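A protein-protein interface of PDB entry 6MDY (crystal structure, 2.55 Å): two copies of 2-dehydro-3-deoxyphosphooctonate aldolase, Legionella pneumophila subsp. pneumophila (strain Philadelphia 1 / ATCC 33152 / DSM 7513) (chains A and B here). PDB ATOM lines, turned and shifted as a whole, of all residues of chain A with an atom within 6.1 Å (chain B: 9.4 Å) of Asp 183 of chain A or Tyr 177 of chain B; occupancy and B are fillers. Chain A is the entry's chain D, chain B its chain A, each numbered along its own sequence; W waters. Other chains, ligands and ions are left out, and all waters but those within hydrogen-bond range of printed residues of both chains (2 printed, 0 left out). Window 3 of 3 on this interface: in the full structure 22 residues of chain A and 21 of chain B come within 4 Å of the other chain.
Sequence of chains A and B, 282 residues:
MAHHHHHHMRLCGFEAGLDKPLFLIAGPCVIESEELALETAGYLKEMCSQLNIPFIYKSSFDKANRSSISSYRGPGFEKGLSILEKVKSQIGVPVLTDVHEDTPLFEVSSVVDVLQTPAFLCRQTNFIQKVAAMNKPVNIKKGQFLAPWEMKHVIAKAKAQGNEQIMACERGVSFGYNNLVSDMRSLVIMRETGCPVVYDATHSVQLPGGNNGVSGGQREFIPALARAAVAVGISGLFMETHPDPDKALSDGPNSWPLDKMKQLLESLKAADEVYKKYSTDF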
ATOM      1  N   LYS A 142      30.073  -2.751  24.335  1.00  0.00           N
ATOM      2  CA  LYS A 142      28.872  -3.413  23.841  1.00  0.00           C
ATOM      3  C   LYS A 142      29.189  -4.197  22.577  1.00  0.00           C
ATOM      4  O   LYS A 142      29.737  -3.647  21.617  1.00  0.00           O
ATOM      5  CB  LYS A 142      27.770  -2.395  23.556  1.00  0.00           C
ATOM      6  CG  LYS A 142      26.642  -2.954  22.713  1.00  0.00           C
ATOM      7  CD  LYS A 142      25.305  -2.340  23.100  1.00  0.00           C
ATOM      8  CE  LYS A 142      25.005  -1.079  22.294  1.00  0.00           C
ATOM      9  NZ  LYS A 142      25.047  -1.309  20.816  1.00  0.00           N
ATOM     10  N   LEU A 146      24.668  -7.022  19.951  1.00  0.00           N
ATOM     11  CA  LEU A 146      23.762  -6.740  21.053  1.00  0.00           C
ATOM     12  C   LEU A 146      22.824  -5.600  20.692  1.00  0.00           C
ATOM     13  O   LEU A 146      23.231  -4.614  20.072  1.00  0.00           O
ATOM     14  CB  LEU A 146      24.530  -6.380  22.325  1.00  0.00           C
ATOM     15  CG  LEU A 146      24.733  -7.508  23.337  1.00  0.00           C
ATOM     16  CD1 LEU A 146      25.901  -8.363  22.946  1.00  0.00           C
ATOM     17  CD2 LEU A 146      24.956  -6.904  24.704  1.00  0.00           C
ATOM     18  N   ALA A 147      21.587  -5.754  21.054  1.00  0.00           N
ATOM     19  CA  ALA A 147      20.670  -4.639  21.028  1.00  0.00           C
ATOM     20  C   ALA A 147      20.884  -3.781  22.277  1.00  0.00           C
ATOM     21  O   ALA A 147      21.332  -4.287  23.309  1.00  0.00           O
ATOM     22  CB  ALA A 147      19.229  -5.139  20.968  1.00  0.00           C
ATOM     23  N   PRO A 148      20.616  -2.470  22.195  1.00  0.00           N
ATOM     24  CA  PRO A 148      20.851  -1.605  23.367  1.00  0.00           C
ATOM     25  C   PRO A 148      20.129  -2.062  24.629  1.00  0.00           C
ATOM     26  O   PRO A 148      20.702  -1.992  25.724  1.00  0.00           O
ATOM     27  CB  PRO A 148      20.339  -0.238  22.897  1.00  0.00           C
ATOM     28  CG  PRO A 148      20.432  -0.288  21.427  1.00  0.00           C
ATOM     29  CD  PRO A 148      20.174  -1.703  21.021  1.00  0.00           C
ATOM     30  N   TRP A 149      18.888  -2.531  24.518  1.00  0.00           N
ATOM     31  CA  TRP A 149      18.199  -2.973  25.720  1.00  0.00           C
ATOM     32  C   TRP A 149      18.869  -4.187  26.354  1.00  0.00           C
ATOM     33  O   TRP A 149      18.714  -4.398  27.563  1.00  0.00           O
ATOM     34  CB  TRP A 149      16.729  -3.281  25.408  1.00  0.00           C
ATOM     35  CG  TRP A 149      16.534  -4.510  24.586  1.00  0.00           C
ATOM     36  CD1 TRP A 149      16.382  -4.573  23.230  1.00  0.00           C
ATOM     37  CD2 TRP A 149      16.475  -5.868  25.061  1.00  0.00           C
ATOM     38  NE1 TRP A 149      16.234  -5.882  22.832  1.00  0.00           N
ATOM     39  CE2 TRP A 149      16.288  -6.696  23.934  1.00  0.00           C
ATOM     40  CE3 TRP A 149      16.560  -6.462  26.329  1.00  0.00           C
ATOM     41  CZ2 TRP A 149      16.185  -8.085  24.036  1.00  0.00           C
ATOM     42  CZ3 TRP A 149      16.459  -7.844  26.427  1.00  0.00           C
ATOM     43  CH2 TRP A 149      16.272  -8.638  25.286  1.00  0.00           C
ATOM     44  N   GLU A 170      29.827   2.161  23.657  1.00  0.00           N
ATOM     45  CA  GLU A 170      29.187   1.857  22.382  1.00  0.00           C
ATOM     46  C   GLU A 170      30.237   1.782  21.281  1.00  0.00           C
ATOM     47  O   GLU A 170      31.094   2.666  21.191  1.00  0.00           O
ATOM     48  CB  GLU A 170      28.153   2.936  22.061  1.00  0.00           C
ATOM     49  CG  GLU A 170      27.815   3.065  20.594  1.00  0.00           C
ATOM     50  CD  GLU A 170      27.014   1.888  20.088  1.00  0.00           C
ATOM     51  OE1 GLU A 170      26.134   1.399  20.833  1.00  0.00           O
ATOM     52  OE2 GLU A 170      27.274   1.451  18.952  1.00  0.00           O
ATOM     53  N   GLY A 172      29.264   0.375  17.872  1.00  0.00           N
ATOM     54  CA  GLY A 172      28.639   0.039  16.613  1.00  0.00           C
ATOM     55  C   GLY A 172      27.969  -1.325  16.657  1.00  0.00           C
ATOM     56  O   GLY A 172      28.279  -2.181  17.488  1.00  0.00           O
ATOM     57  N   VAL A 173      27.018  -1.521  15.744  1.00  0.00           N
ATOM     58  CA  VAL A 173      26.322  -2.790  15.626  1.00  0.00           C
ATOM     59  C   VAL A 173      26.399  -3.260  14.184  1.00  0.00           C
ATOM     60  O   VAL A 173      26.472  -2.463  13.242  1.00  0.00           O
ATOM     61  CB  VAL A 173      24.856  -2.708  16.110  1.00  0.00           C
ATOM     62  CG1 VAL A 173      24.818  -2.713  17.631  1.00  0.00           C
ATOM     63  CG2 VAL A 173      24.180  -1.477  15.553  1.00  0.00           C
ATOM     64  N   VAL A 181      27.291  -0.031  11.851  1.00  0.00           N
ATOM     65  CA  VAL A 181      26.546   1.219  11.823  1.00  0.00           C
ATOM     66  C   VAL A 181      26.466   1.752  13.246  1.00  0.00           C
ATOM     67  O   VAL A 181      26.386   0.985  14.211  1.00  0.00           O
ATOM     68  CB  VAL A 181      25.143   1.057  11.192  1.00  0.00           C
ATOM     69  CG1 VAL A 181      24.182   0.341  12.135  1.00  0.00           C
ATOM     70  CG2 VAL A 181      24.585   2.413  10.795  1.00  0.00           C
ATOM     71  N   SER A 182      26.522   3.061  13.376  1.00  0.00           N
ATOM     72  CA  SER A 182      26.442   3.709  14.676  1.00  0.00           C
ATOM     73  C   SER A 182      25.004   4.189  14.869  1.00  0.00           C
ATOM     74  O   SER A 182      24.630   5.262  14.394  1.00  0.00           O
ATOM     75  CB  SER A 182      27.451   4.847  14.745  1.00  0.00           C
ATOM     76  OG  SER A 182      27.859   5.072  16.072  1.00  0.00           O
ATOM     77  N   ASP A 183      24.196   3.391  15.566  1.00  0.00           N
ATOM     78  CA  ASP A 183      22.812   3.757  15.870  1.00  0.00           C
ATOM     79  C   ASP A 183      22.817   4.699  17.062  1.00  0.00           C
ATOM     80  O   ASP A 183      22.948   4.266  18.211  1.00  0.00           O
ATOM     81  CB  ASP A 183      21.969   2.515  16.148  1.00  0.00           C
ATOM     82  CG  ASP A 183      20.483   2.838  16.372  1.00  0.00           C
ATOM     83  OD1 ASP A 183      20.101   4.027  16.469  1.00  0.00           O
ATOM     84  OD2 ASP A 183      19.678   1.879  16.420  1.00  0.00           O
ATOM     85  N   MET A 184      22.616   5.992  16.790  1.00  0.00           N
ATOM     86  CA  MET A 184      22.710   7.000  17.839  1.00  0.00           C
ATOM     87  C   MET A 184      21.649   6.820  18.913  1.00  0.00           C
ATOM     88  O   MET A 184      21.811   7.344  20.023  1.00  0.00           O
ATOM     89  CB  MET A 184      22.606   8.404  17.231  1.00  0.00           C
ATOM     90  CG  MET A 184      23.737   8.744  16.265  1.00  0.00           C
ATOM     91  SD  MET A 184      25.358   8.755  17.065  1.00  0.00           S
ATOM     92  CE  MET A 184      26.440   8.286  15.714  1.00  0.00           C
ATOM     93  N   ARG A 185      20.575   6.081  18.617  1.00  0.00           N
ATOM     94  CA  ARG A 185      19.566   5.818  19.638  1.00  0.00           C
ATOM     95  C   ARG A 185      20.152   5.083  20.836  1.00  0.00           C
ATOM     96  O   ARG A 185      19.696   5.291  21.967  1.00  0.00           O
ATOM     97  CB  ARG A 185      18.412   5.003  19.043  1.00  0.00           C
ATOM     98  CG  ARG A 185      17.597   5.742  17.983  1.00  0.00           C
ATOM     99  CD  ARG A 185      16.606   4.803  17.306  1.00  0.00           C
ATOM    100  NE  ARG A 185      17.294   3.735  16.574  1.00  0.00           N
ATOM    101  CZ  ARG A 185      16.696   2.858  15.772  1.00  0.00           C
ATOM    102  NH1 ARG A 185      15.387   2.907  15.586  1.00  0.00           N
ATOM    103  NH2 ARG A 185      17.409   1.922  15.161  1.00  0.00           N
ATOM    104  N   SER A 186      21.160   4.227  20.617  1.00  0.00           N
ATOM    105  CA  SER A 186      21.730   3.467  21.724  1.00  0.00           C
ATOM    106  C   SER A 186      22.396   4.385  22.747  1.00  0.00           C
ATOM    107  O   SER A 186      22.390   4.085  23.949  1.00  0.00           O
ATOM    108  CB  SER A 186      22.700   2.403  21.200  1.00  0.00           C
ATOM    109  OG  SER A 186      24.044   2.816  21.310  1.00  0.00           O
ATOM    110  N   LEU A 187      22.959   5.513  22.302  1.00  0.00           N
ATOM    111  CA  LEU A 187      23.546   6.443  23.259  1.00  0.00           C
ATOM    112  C   LEU A 187      22.493   6.952  24.226  1.00  0.00           C
ATOM    113  O   LEU A 187      22.805   7.254  25.386  1.00  0.00           O
ATOM    114  CB  LEU A 187      24.208   7.617  22.539  1.00  0.00           C
ATOM    115  CG  LEU A 187      25.316   7.270  21.542  1.00  0.00           C
ATOM    116  CD1 LEU A 187      25.825   8.533  20.866  1.00  0.00           C
ATOM    117  CD2 LEU A 187      26.457   6.504  22.217  1.00  0.00           C
ATOM    118  N   VAL B 173      23.455 -15.365  11.210  1.00  0.00           N
ATOM    119  CA  VAL B 173      24.107 -14.065  11.137  1.00  0.00           C
ATOM    120  C   VAL B 173      23.133 -13.019  11.662  1.00  0.00           C
ATOM    121  O   VAL B 173      21.911 -13.148  11.516  1.00  0.00           O
ATOM    122  CB  VAL B 173      24.575 -13.741   9.694  1.00  0.00           C
ATOM    123  CG1 VAL B 173      23.393 -13.570   8.766  1.00  0.00           C
ATOM    124  CG2 VAL B 173      25.421 -12.486   9.667  1.00  0.00           C
ATOM    125  N   SER B 174      23.677 -11.990  12.304  1.00  0.00           N
ATOM    126  CA  SER B 174      22.837 -10.953  12.891  1.00  0.00           C
ATOM    127  C   SER B 174      22.045 -10.227  11.813  1.00  0.00           C
ATOM    128  O   SER B 174      22.574  -9.871  10.759  1.00  0.00           O
ATOM    129  CB  SER B 174      23.686  -9.956  13.678  1.00  0.00           C
ATOM    130  OG  SER B 174      24.265 -10.581  14.802  1.00  0.00           O
ATOM    131  N   PHE B 175      20.771  -9.986  12.099  1.00  0.00           N
ATOM    132  CA  PHE B 175      19.845  -9.326  11.185  1.00  0.00           C
ATOM    133  C   PHE B 175      19.123  -8.261  12.004  1.00  0.00           C
ATOM    134  O   PHE B 175      18.108  -8.547  12.643  1.00  0.00           O
ATOM    135  CB  PHE B 175      18.872 -10.339  10.559  1.00  0.00           C
ATOM    136  CG  PHE B 175      17.995  -9.749   9.493  1.00  0.00           C
ATOM    137  CD1 PHE B 175      18.556  -9.135   8.388  1.00  0.00           C
ATOM    138  CD2 PHE B 175      16.615  -9.799   9.591  1.00  0.00           C
ATOM    139  CE1 PHE B 175      17.757  -8.575   7.406  1.00  0.00           C
ATOM    140  CE2 PHE B 175      15.814  -9.247   8.600  1.00  0.00           C
ATOM    141  CZ  PHE B 175      16.385  -8.639   7.513  1.00  0.00           C
ATOM    142  N   GLY B 176      19.654  -7.040  11.993  1.00  0.00           N
ATOM    143  CA  GLY B 176      19.090  -6.019  12.853  1.00  0.00           C
ATOM    144  C   GLY B 176      19.277  -6.387  14.315  1.00  0.00           C
ATOM    145  O   GLY B 176      20.224  -7.079  14.698  1.00  0.00           O
ATOM    146  N   TYR B 177      18.345  -5.930  15.143  1.00  0.00           N
ATOM    147  CA  TYR B 177      18.356  -6.234  16.567  1.00  0.00           C
ATOM    148  C   TYR B 177      17.556  -7.498  16.868  1.00  0.00           C
ATOM    149  O   TYR B 177      16.472  -7.708  16.320  1.00  0.00           O
ATOM    150  CB  TYR B 177      17.778  -5.067  17.364  1.00  0.00           C
ATOM    151  CG  TYR B 177      18.619  -3.818  17.336  1.00  0.00           C
ATOM    152  CD1 TYR B 177      19.994  -3.862  17.595  1.00  0.00           C
ATOM    153  CD2 TYR B 177      18.036  -2.589  17.057  1.00  0.00           C
ATOM    154  CE1 TYR B 177      20.760  -2.701  17.568  1.00  0.00           C
ATOM    155  CE2 TYR B 177      18.780  -1.437  17.027  1.00  0.00           C
ATOM    156  CZ  TYR B 177      20.132  -1.488  17.280  1.00  0.00           C
ATOM    157  OH  TYR B 177      20.833  -0.313  17.243  1.00  0.00           O
ATOM    158  N   ASN B 178      18.109  -8.342  17.743  1.00  0.00           N
ATOM    159  CA  ASN B 178      17.386  -9.480  18.324  1.00  0.00           C
ATOM    160  C   ASN B 178      16.811 -10.406  17.256  1.00  0.00           C
ATOM    161  O   ASN B 178      15.675 -10.873  17.358  1.00  0.00           O
ATOM    162  CB  ASN B 178      16.279  -8.999  19.259  1.00  0.00           C
ATOM    163  CG  ASN B 178      16.810  -8.147  20.381  1.00  0.00           C
ATOM    164  OD1 ASN B 178      16.420  -6.987  20.526  1.00  0.00           O
ATOM    165  ND2 ASN B 178      17.709  -8.713  21.186  1.00  0.00           N
ATOM    166  N   ASN B 179      17.613 -10.711  16.246  1.00  0.00           N
ATOM    167  CA  ASN B 179      17.142 -11.536  15.149  1.00  0.00           C
ATOM    168  C   ASN B 179      18.344 -12.124  14.431  1.00  0.00           C
ATOM    169  O   ASN B 179      19.305 -11.406  14.137  1.00  0.00           O
ATOM    170  CB  ASN B 179      16.281 -10.721  14.181  1.00  0.00           C
ATOM    171  CG  ASN B 179      15.418 -11.598  13.298  1.00  0.00           C
ATOM    172  OD1 ASN B 179      15.922 -12.393  12.498  1.00  0.00           O
ATOM    173  ND2 ASN B 179      14.109 -11.474  13.455  1.00  0.00           N
ATOM    174  N   LEU B 180      18.288 -13.422  14.160  1.00  0.00           N
ATOM    175  CA  LEU B 180      19.291 -14.106  13.364  1.00  0.00           C
ATOM    176  C   LEU B 180      18.645 -14.596  12.081  1.00  0.00           C
ATOM    177  O   LEU B 180      17.527 -15.124  12.104  1.00  0.00           O
ATOM    178  CB  LEU B 180      19.889 -15.294  14.127  1.00  0.00           C
ATOM    179  CG  LEU B 180      20.761 -14.946  15.332  1.00  0.00           C
ATOM    180  CD1 LEU B 180      21.238 -16.211  16.019  1.00  0.00           C
ATOM    181  CD2 LEU B 180      21.943 -14.061  14.918  1.00  0.00           C
ATOM    182  N   VAL B 181      19.334 -14.408  10.960  1.00  0.00           N
ATOM    183  CA  VAL B 181      18.858 -14.910   9.679  1.00  0.00           C
ATOM    184  C   VAL B 181      19.841 -15.963   9.195  1.00  0.00           C
ATOM    185  O   VAL B 181      21.048 -15.867   9.446  1.00  0.00           O
ATOM    186  CB  VAL B 181      18.662 -13.801   8.626  1.00  0.00           C
ATOM    187  CG1 VAL B 181      19.969 -13.199   8.225  1.00  0.00           C
ATOM    188  CG2 VAL B 181      17.954 -14.368   7.385  1.00  0.00           C
ATOM    189  N   GLN B 206      17.117 -18.941  17.144  1.00  0.00           N
ATOM    190  CA  GLN B 206      17.264 -18.362  18.513  1.00  0.00           C
ATOM    191  C   GLN B 206      17.083 -16.844  18.671  1.00  0.00           C
ATOM    192  O   GLN B 206      17.765 -16.050  18.015  1.00  0.00           O
ATOM    193  CB  GLN B 206      18.642 -18.695  19.097  1.00  0.00           C
HETATM  194  O   HOH W   1      23.233  -0.342  18.961  1.00  0.00           O
HETATM  195  O   HOH W   2      20.705  -7.655  18.641  1.00  0.00           O
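The side-chain carboxylate (OD2) of Asp 183 of chain A lies within hydrogen-bond range of the side-chain hydroxyl (OH) of Tyr 177 of chain B (2.6 Å). The side-chain amide oxygen of Asn 178 of chain B sits at hydrogen-bond distance from the indole nitrogen of Trp 149 of chain A (2.6 Å).
O of Val 173 of chain A sits at hydrogen-bond distance from N of Val 181 of chain A (2.9 Å). NH2 of Arg 185 of chain A is in salt-bridge range of OD2 of Asp 183 of chain A, at 2.6 Å.
CD1 of Tyr 177 of chain B touches CA of Ala 147 of chain A, 3.6 Å away. CB of Ala 147 of chain A touches OD1 of Asn 178 of chain B, at 3.4 Å. Pro 148 of chain A touches Tyr 177 of chain B (CD to CE1, 3.6 Å). Val 173 of chain A touches Tyr 177 of chain B (CG2 to OH, 3.9 Å).
Asp 183 of chain A touches just one residue of chain B: Tyr 177. Of the printed residues of chain A, Tyr 177 of chain B touches Ala 147 (3.6 Å), Pro 148 (3.6 Å), Val 173 (3.9 Å) and Asp 183 (2.6 Å). Printed residues of chain B within 4 Å of Val 173 of chain A: Tyr 177. Of the printed residues of chain A, Asn 178 of chain B touches Ala 147 and Trp 149. Gly 172 of chain A touches none of the printed residues of chain B. Lys 142 of chain A touches none of the printed residues of chain B. The nearest residue of chain B that does not touch Asp 183 of chain A is Gly 176 of chain B (8.5 Å). The nearest printed residue of chain A that does not touch Tyr 177 of chain B is Leu 146 of chain A (4.004 Å).
Of the 10 printed residues of chain B, 2 touch a printed residue of chain A. Hydrophobic or aromatic side chains of chain B that line the printed part of chain A: Tyr 177. Among the printed residues, 6 pairs touch across the chains. Among the printed residues, no Asp or Glu carboxylate lies within 4 Å of a Lys or Arg side-chain nitrogen of the other chain.
Positions printed for both chains: 173 and 181.
Water W1 lies within hydrogen-bond range of the side-chain amino group (NZ) of Lys 142 of chain A (2.8 Å) and the side-chain hydroxyl (OH) of Tyr 177 of chain B (3.0 Å). Water W2 bridges the backbone NH (N) of Asn 178 of chain B (2.8 Å) and the backbone NH (N) of Ala 147 of chain A (3.2 Å).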
